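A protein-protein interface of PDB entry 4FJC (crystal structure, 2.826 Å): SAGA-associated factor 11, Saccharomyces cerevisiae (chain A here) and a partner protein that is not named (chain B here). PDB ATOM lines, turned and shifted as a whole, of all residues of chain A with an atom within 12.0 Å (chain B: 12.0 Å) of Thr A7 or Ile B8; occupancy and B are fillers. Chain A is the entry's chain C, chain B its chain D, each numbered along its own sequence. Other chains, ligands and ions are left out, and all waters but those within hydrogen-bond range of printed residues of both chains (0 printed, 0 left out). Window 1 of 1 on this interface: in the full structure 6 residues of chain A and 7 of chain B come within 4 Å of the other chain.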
ATOM      1  N   GLU A   3       9.707  20.632 -12.580  1.00  0.00           N
ATOM      2  CA  GLU A   3      10.149  19.312 -13.117  1.00  0.00           C
ATOM      3  C   GLU A   3      11.636  19.070 -12.799  1.00  0.00           C
ATOM      4  O   GLU A   3      11.956  18.526 -11.736  1.00  0.00           O
ATOM      5  CB  GLU A   3       9.857  19.233 -14.630  1.00  0.00           C
ATOM      6  CG  GLU A   3      10.240  17.919 -15.312  1.00  0.00           C
ATOM      7  CD  GLU A   3      10.491  18.076 -16.806  1.00  0.00           C
ATOM      8  OE1 GLU A   3      11.116  17.167 -17.404  1.00  0.00           O
ATOM      9  OE2 GLU A   3      10.070  19.106 -17.385  1.00  0.00           O
ATOM     10  N   GLU A   4      12.533  19.483 -13.702  1.00  0.00           N
ATOM     11  CA  GLU A   4      13.969  19.213 -13.563  1.00  0.00           C
ATOM     12  C   GLU A   4      14.853  20.386 -13.971  1.00  0.00           C
ATOM     13  O   GLU A   4      14.409  21.325 -14.637  1.00  0.00           O
ATOM     14  CB  GLU A   4      14.371  17.966 -14.369  1.00  0.00           C
ATOM     15  CG  GLU A   4      13.785  16.652 -13.852  1.00  0.00           C
ATOM     16  CD  GLU A   4      14.339  16.211 -12.501  1.00  0.00           C
ATOM     17  OE1 GLU A   4      14.638  17.065 -11.638  1.00  0.00           O
ATOM     18  OE2 GLU A   4      14.460  14.988 -12.296  1.00  0.00           O
ATOM     19  N   THR A   5      16.118  20.295 -13.567  1.00  0.00           N
ATOM     20  CA  THR A   5      17.080  21.394 -13.672  1.00  0.00           C
ATOM     21  C   THR A   5      17.516  21.682 -15.110  1.00  0.00           C
ATOM     22  O   THR A   5      18.086  20.806 -15.776  1.00  0.00           O
ATOM     23  CB  THR A   5      18.336  21.085 -12.818  1.00  0.00           C
ATOM     24  OG1 THR A   5      17.984  21.102 -11.426  1.00  0.00           O
ATOM     25  CG2 THR A   5      19.453  22.097 -13.074  1.00  0.00           C
ATOM     26  N   ILE A   6      17.255  22.910 -15.573  1.00  0.00           N
ATOM     27  CA  ILE A   6      17.800  23.384 -16.847  1.00  0.00           C
ATOM     28  C   ILE A   6      19.081  24.204 -16.597  1.00  0.00           C
ATOM     29  O   ILE A   6      19.051  25.313 -16.088  1.00  0.00           O
ATOM     30  CB  ILE A   6      16.737  24.102 -17.729  1.00  0.00           C
ATOM     31  CG1 ILE A   6      16.635  25.603 -17.449  1.00  0.00           C
ATOM     32  CG2 ILE A   6      15.375  23.440 -17.560  1.00  0.00           C
ATOM     33  CD1 ILE A   6      15.508  26.269 -18.203  1.00  0.00           C
ATOM     34  N   THR A   7      20.217  23.616 -16.938  1.00  0.00           N
ATOM     35  CA  THR A   7      21.513  24.231 -16.692  1.00  0.00           C
ATOM     36  C   THR A   7      22.100  24.833 -17.978  1.00  0.00           C
ATOM     37  O   THR A   7      21.547  24.692 -19.070  1.00  0.00           O
ATOM     38  CB  THR A   7      22.516  23.216 -16.054  1.00  0.00           C
ATOM     39  OG1 THR A   7      23.867  23.523 -16.441  1.00  0.00           O
ATOM     40  CG2 THR A   7      22.222  21.786 -16.469  1.00  0.00           C
ATOM     41  N   ILE A   8      23.223  25.523 -17.820  1.00  0.00           N
ATOM     42  CA  ILE A   8      24.023  25.949 -18.956  1.00  0.00           C
ATOM     43  C   ILE A   8      24.483  24.740 -19.764  1.00  0.00           C
ATOM     44  O   ILE A   8      24.460  24.778 -20.993  1.00  0.00           O
ATOM     45  CB  ILE A   8      25.257  26.758 -18.507  1.00  0.00           C
ATOM     46  CG1 ILE A   8      24.855  28.202 -18.190  1.00  0.00           C
ATOM     47  CG2 ILE A   8      26.338  26.726 -19.582  1.00  0.00           C
ATOM     48  CD1 ILE A   8      26.036  29.150 -18.048  1.00  0.00           C
ATOM     49  N   ASP A   9      24.904  23.681 -19.068  1.00  0.00           N
ATOM     50  CA  ASP A   9      25.307  22.424 -19.718  1.00  0.00           C
ATOM     51  C   ASP A   9      24.153  21.769 -20.469  1.00  0.00           C
ATOM     52  O   ASP A   9      24.352  21.258 -21.572  1.00  0.00           O
ATOM     53  CB  ASP A   9      25.858  21.410 -18.695  1.00  0.00           C
ATOM     54  CG  ASP A   9      27.295  21.720 -18.242  1.00  0.00           C
ATOM     55  OD1 ASP A   9      27.970  22.593 -18.856  1.00  0.00           O
ATOM     56  OD2 ASP A   9      27.752  21.068 -17.261  1.00  0.00           O
ATOM     57  N   SER A  10      22.953  21.776 -19.877  1.00  0.00           N
ATOM     58  CA  SER A  10      21.831  21.033 -20.455  1.00  0.00           C
ATOM     59  C   SER A  10      21.270  21.729 -21.690  1.00  0.00           C
ATOM     60  O   SER A  10      21.029  21.062 -22.685  1.00  0.00           O
ATOM     61  CB  SER A  10      20.719  20.770 -19.435  1.00  0.00           C
ATOM     62  OG  SER A  10      19.913  21.913 -19.252  1.00  0.00           O
ATOM     63  N   ILE A  11      21.059  23.044 -21.637  1.00  0.00           N
ATOM     64  CA  ILE A  11      20.575  23.757 -22.811  1.00  0.00           C
ATOM     65  C   ILE A  11      21.602  23.665 -23.920  1.00  0.00           C
ATOM     66  O   ILE A  11      21.247  23.509 -25.089  1.00  0.00           O
ATOM     67  CB  ILE A  11      20.273  25.253 -22.543  1.00  0.00           C
ATOM     68  CG1 ILE A  11      18.932  25.422 -21.818  1.00  0.00           C
ATOM     69  CG2 ILE A  11      20.210  26.041 -23.848  1.00  0.00           C
ATOM     70  CD1 ILE A  11      17.726  24.917 -22.590  1.00  0.00           C
ATOM     71  N   SER A  12      22.876  23.764 -23.550  1.00  0.00           N
ATOM     72  CA  SER A  12      23.963  23.679 -24.525  1.00  0.00           C
ATOM     73  C   SER A  12      23.946  22.351 -25.272  1.00  0.00           C
ATOM     74  O   SER A  12      24.140  22.320 -26.488  1.00  0.00           O
ATOM     75  CB  SER A  12      25.321  23.851 -23.848  1.00  0.00           C
ATOM     76  OG  SER A  12      25.565  25.194 -23.527  1.00  0.00           O
ATOM     77  N   ASN A  13      23.746  21.262 -24.525  1.00  0.00           N
ATOM     78  CA  ASN A  13      23.692  19.919 -25.081  1.00  0.00           C
ATOM     79  C   ASN A  13      22.421  19.787 -25.914  1.00  0.00           C
ATOM     80  O   ASN A  13      22.381  19.047 -26.882  1.00  0.00           O
ATOM     81  CB  ASN A  13      23.736  18.862 -23.962  1.00  0.00           C
ATOM     82  CG  ASN A  13      25.154  18.594 -23.425  1.00  0.00           C
ATOM     83  OD1 ASN A  13      26.092  18.341 -24.178  1.00  0.00           O
ATOM     84  ND2 ASN A  13      25.292  18.598 -22.111  1.00  0.00           N
ATOM     85  N   GLY A  14      21.390  20.539 -25.564  1.00  0.00           N
ATOM     86  CA  GLY A  14      20.180  20.584 -26.373  1.00  0.00           C
ATOM     87  C   GLY A  14      20.413  21.198 -27.734  1.00  0.00           C
ATOM     88  O   GLY A  14      19.921  20.726 -28.740  1.00  0.00           O
ATOM     89  N   ILE A  15      21.180  22.264 -27.767  1.00  0.00           N
ATOM     90  CA  ILE A  15      21.469  22.917 -29.013  1.00  0.00           C
ATOM     91  C   ILE A  15      22.381  22.045 -29.892  1.00  0.00           C
ATOM     92  O   ILE A  15      22.207  21.980 -31.129  1.00  0.00           O
ATOM     93  CB  ILE A  15      22.096  24.276 -28.744  1.00  0.00           C
ATOM     94  CG1 ILE A  15      21.086  25.153 -28.018  1.00  0.00           C
ATOM     95  CG2 ILE A  15      22.476  24.926 -30.044  1.00  0.00           C
ATOM     96  CD1 ILE A  15      21.685  26.375 -27.381  1.00  0.00           C
ATOM     97  N   LEU A  16      23.331  21.360 -29.252  1.00  0.00           N
ATOM     98  CA  LEU A  16      24.232  20.446 -29.976  1.00  0.00           C
ATOM     99  C   LEU A  16      23.515  19.242 -30.573  1.00  0.00           C
ATOM    100  O   LEU A  16      23.870  18.796 -31.665  1.00  0.00           O
ATOM    101  CB  LEU A  16      25.384  19.944 -29.092  1.00  0.00           C
ATOM    102  CG  LEU A  16      26.346  19.018 -29.870  1.00  0.00           C
ATOM    103  CD1 LEU A  16      26.868  19.689 -31.129  1.00  0.00           C
ATOM    104  CD2 LEU A  16      27.497  18.532 -29.011  1.00  0.00           C
ATOM    105  N   ASP B   5      26.242  22.621 -15.398  1.00  0.00           N
ATOM    106  CA  ASP B   5      27.174  23.531 -14.655  1.00  0.00           C
ATOM    107  C   ASP B   5      26.359  24.449 -13.735  1.00  0.00           C
ATOM    108  O   ASP B   5      26.261  24.183 -12.537  1.00  0.00           O
ATOM    109  CB  ASP B   5      28.084  24.319 -15.639  1.00  0.00           C
ATOM    110  CG  ASP B   5      29.089  25.259 -14.935  1.00  0.00           C
ATOM    111  OD1 ASP B   5      28.832  25.680 -13.786  1.00  0.00           O
ATOM    112  OD2 ASP B   5      30.134  25.592 -15.552  1.00  0.00           O
ATOM    113  N   ALA B   6      25.753  25.496 -14.302  1.00  0.00           N
ATOM    114  CA  ALA B   6      25.019  26.508 -13.535  1.00  0.00           C
ATOM    115  C   ALA B   6      23.544  26.562 -13.963  1.00  0.00           C
ATOM    116  O   ALA B   6      23.244  26.568 -15.158  1.00  0.00           O
ATOM    117  CB  ALA B   6      25.678  27.869 -13.722  1.00  0.00           C
ATOM    118  N   GLU B   7      22.639  26.609 -12.985  1.00  0.00           N
ATOM    119  CA  GLU B   7      21.193  26.642 -13.235  1.00  0.00           C
ATOM    120  C   GLU B   7      20.757  28.001 -13.816  1.00  0.00           C
ATOM    121  O   GLU B   7      21.433  29.010 -13.595  1.00  0.00           O
ATOM    122  CB  GLU B   7      20.456  26.368 -11.928  1.00  0.00           C
ATOM    123  CG  GLU B   7      18.973  26.044 -12.069  1.00  0.00           C
ATOM    124  CD  GLU B   7      18.194  26.261 -10.773  1.00  0.00           C
ATOM    125  OE1 GLU B   7      18.834  26.402  -9.700  1.00  0.00           O
ATOM    126  OE2 GLU B   7      16.936  26.295 -10.825  1.00  0.00           O
ATOM    127  N   ILE B   8      19.635  28.030 -14.542  1.00  0.00           N
ATOM    128  CA  ILE B   8      19.254  29.203 -15.322  1.00  0.00           C
ATOM    129  C   ILE B   8      17.906  29.788 -14.948  1.00  0.00           C
ATOM    130  O   ILE B   8      16.888  29.130 -15.089  1.00  0.00           O
ATOM    131  CB  ILE B   8      19.222  28.872 -16.820  1.00  0.00           C
ATOM    132  CG1 ILE B   8      20.617  28.406 -17.285  1.00  0.00           C
ATOM    133  CG2 ILE B   8      18.734  30.083 -17.610  1.00  0.00           C
ATOM    134  CD1 ILE B   8      20.865  28.500 -18.781  1.00  0.00           C
ATOM    135  N   LYS B   9      17.922  31.056 -14.526  1.00  0.00           N
ATOM    136  CA  LYS B   9      16.731  31.806 -14.090  1.00  0.00           C
ATOM    137  C   LYS B   9      15.904  32.295 -15.268  1.00  0.00           C
ATOM    138  O   LYS B   9      14.679  32.349 -15.189  1.00  0.00           O
ATOM    139  CB  LYS B   9      17.140  33.021 -13.233  1.00  0.00           C
ATOM    140  CG  LYS B   9      16.010  33.586 -12.355  1.00  0.00           C
ATOM    141  CD  LYS B   9      16.141  35.077 -11.962  1.00  0.00           C
ATOM    142  CE  LYS B   9      15.344  36.045 -12.850  1.00  0.00           C
ATOM    143  NZ  LYS B   9      16.179  36.711 -13.901  1.00  0.00           N
ATOM    144  N   GLY B  10      16.577  32.687 -16.346  1.00  0.00           N
ATOM    145  CA  GLY B  10      15.896  33.087 -17.576  1.00  0.00           C
ATOM    146  C   GLY B  10      16.832  33.877 -18.449  1.00  0.00           C
ATOM    147  O   GLY B  10      17.991  34.037 -18.092  1.00  0.00           O
ATOM    148  N   ILE B  11      16.345  34.377 -19.584  1.00  0.00           N
ATOM    149  CA  ILE B  11      17.163  35.211 -20.461  1.00  0.00           C
ATOM    150  C   ILE B  11      17.275  36.598 -19.857  1.00  0.00           C
ATOM    151  O   ILE B  11      16.294  37.122 -19.342  1.00  0.00           O
ATOM    152  CB  ILE B  11      16.539  35.370 -21.865  1.00  0.00           C
ATOM    153  CG1 ILE B  11      16.448  34.022 -22.586  1.00  0.00           C
ATOM    154  CG2 ILE B  11      17.365  36.324 -22.719  1.00  0.00           C
ATOM    155  CD1 ILE B  11      15.686  34.076 -23.893  1.00  0.00           C
ATOM    156  N   LYS B  12      18.451  37.211 -19.933  1.00  0.00           N
ATOM    157  CA  LYS B  12      18.574  38.604 -19.515  1.00  0.00           C
ATOM    158  C   LYS B  12      17.416  39.405 -20.106  1.00  0.00           C
ATOM    159  O   LYS B  12      17.086  39.222 -21.279  1.00  0.00           O
ATOM    160  CB  LYS B  12      19.888  39.214 -19.972  1.00  0.00           C
ATOM    161  CG  LYS B  12      21.085  38.802 -19.137  1.00  0.00           C
ATOM    162  CD  LYS B  12      22.399  39.182 -19.820  1.00  0.00           C
ATOM    163  CE  LYS B  12      23.584  38.473 -19.182  1.00  0.00           C
ATOM    164  NZ  LYS B  12      23.529  38.565 -17.692  1.00  0.00           N
ATOM    165  N   PRO B  13      16.767  40.263 -19.284  1.00  0.00           N
ATOM    166  CA  PRO B  13      15.705  41.175 -19.746  1.00  0.00           C
ATOM    167  C   PRO B  13      16.087  42.096 -20.901  1.00  0.00           C
ATOM    168  O   PRO B  13      15.325  42.221 -21.861  1.00  0.00           O
ATOM    169  CB  PRO B  13      15.386  41.986 -18.495  1.00  0.00           C
ATOM    170  CG  PRO B  13      15.609  41.016 -17.387  1.00  0.00           C
ATOM    171  CD  PRO B  13      16.788  40.175 -17.806  1.00  0.00           C
ATOM    172  N   VAL B  15      18.255  41.666 -23.240  1.00  0.00           N
ATOM    173  CA  VAL B  15      18.347  40.848 -24.454  1.00  0.00           C
ATOM    174  C   VAL B  15      16.952  40.538 -24.996  1.00  0.00           C
ATOM    175  O   VAL B  15      16.723  40.678 -26.200  1.00  0.00           O
ATOM    176  CB  VAL B  15      19.097  39.519 -24.227  1.00  0.00           C
ATOM    177  CG1 VAL B  15      18.920  38.614 -25.428  1.00  0.00           C
ATOM    178  CG2 VAL B  15      20.579  39.752 -23.976  1.00  0.00           C
ATOM    179  N   ILE B  16      16.024  40.148 -24.113  1.00  0.00           N
ATOM    180  CA  ILE B  16      14.650  39.813 -24.525  1.00  0.00           C
ATOM    181  C   ILE B  16      13.979  40.908 -25.337  1.00  0.00           C
ATOM    182  O   ILE B  16      13.259  40.621 -26.300  1.00  0.00           O
ATOM    183  CB  ILE B  16      13.713  39.510 -23.340  1.00  0.00           C
ATOM    184  CG1 ILE B  16      14.019  38.137 -22.747  1.00  0.00           C
ATOM    185  CG2 ILE B  16      12.258  39.527 -23.798  1.00  0.00           C
ATOM    186  CD1 ILE B  16      13.015  37.688 -21.709  1.00  0.00           C
ATOM    187  N   LEU B  21      12.355  38.680 -28.378  1.00  0.00           N
ATOM    188  CA  LEU B  21      12.170  37.247 -28.222  1.00  0.00           C
ATOM    189  C   LEU B  21      10.795  36.853 -27.646  1.00  0.00           C
ATOM    190  O   LEU B  21      10.484  35.664 -27.551  1.00  0.00           O
ATOM    191  CB  LEU B  21      13.308  36.679 -27.373  1.00  0.00           C
ATOM    192  CG  LEU B  21      14.728  36.947 -27.889  1.00  0.00           C
ATOM    193  CD1 LEU B  21      15.763  36.286 -27.010  1.00  0.00           C
ATOM    194  CD2 LEU B  21      14.874  36.452 -29.311  1.00  0.00           C
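The backbone NH (N) of Asp A9 is in hydrogen-bond range of the side-chain hydroxyl (OG1) of Thr A7 (2.8 Å). The backbone carbonyl oxygen (O) of Ile A8 lies within hydrogen-bond range of the side-chain hydroxyl (OG) of Ser A12, 2.8 Å away. OG of Ser A10 is in hydrogen-bond range of N of Thr A7 (2.9 Å). The backbone carbonyl oxygen (O) of Asp A9 is in hydrogen-bond range of the side-chain amide nitrogen (ND2) of Asn A13 (2.9 Å).
The side-chain carboxylate of Asp A9 sits at hydrogen-bond distance from the backbone NH of Asp B5, at 2.9 Å. O of Ile A6 lies within hydrogen-bond range of N of Ile B8. N of Asp B5 lies within hydrogen-bond range of OG1 of Thr A7, at 2.7 Å. The backbone carbonyl oxygen (O) of Ala B6 is in hydrogen-bond range of the backbone NH (N) of Ile A8. O of Ala B6 sits close to OG1 of Thr A7 (3.4 Å).
Among the printed residues, pairs that only touch across the chains: Ile A6 with Glu B7 (3.8 Å), Thr A7 with Ile B8 (3.9 Å) and Ile A8 with Ile B8 (3.9 Å).
Hydrophobic or aromatic side chains of chain B within 4 Å of the printed part of chain A: Ile B8. Along chain B the printed residues that touch a printed residue of chain A span positions 5 to 8. Of the 14 printed residues of chain A, 4 touch a printed residue of chain B. Hydrophobic or aromatic side chains of chain A within 4 Å of the printed part of chain B: Ile A8.
Thr A7 touches just these residues of chain B: Asp B5, Ala B6 and Ile B8. Of chain A, only Ile A6 (3.2 Å), Thr A7 (3.9 Å) and Ile A8 (3.9 Å) come within 4 Å of Ile B8. No residue of chain B comes within 4 Å of Thr A5. Of the printed residues of chain B, Ile A6 touches Glu B7 (3.8 Å) and Ile B8 (3.2 Å). Asp A9 touches just one residue of chain B: Asp B5. Asp B5 touches just these residues of chain A: Thr A7 and Asp A9. Ala B6 touches just these residues of chain A: Thr A7 (3.3 Å) and Ile A8 (2.9 Å). Printed residues of chain A within 4 Å of Glu B7: Ile A6 (3.8 Å). Ser A12 touches none of the printed residues of chain B. The nearest residue of chain A that does not touch Ile B8 is Ile A11 (4.7 Å).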
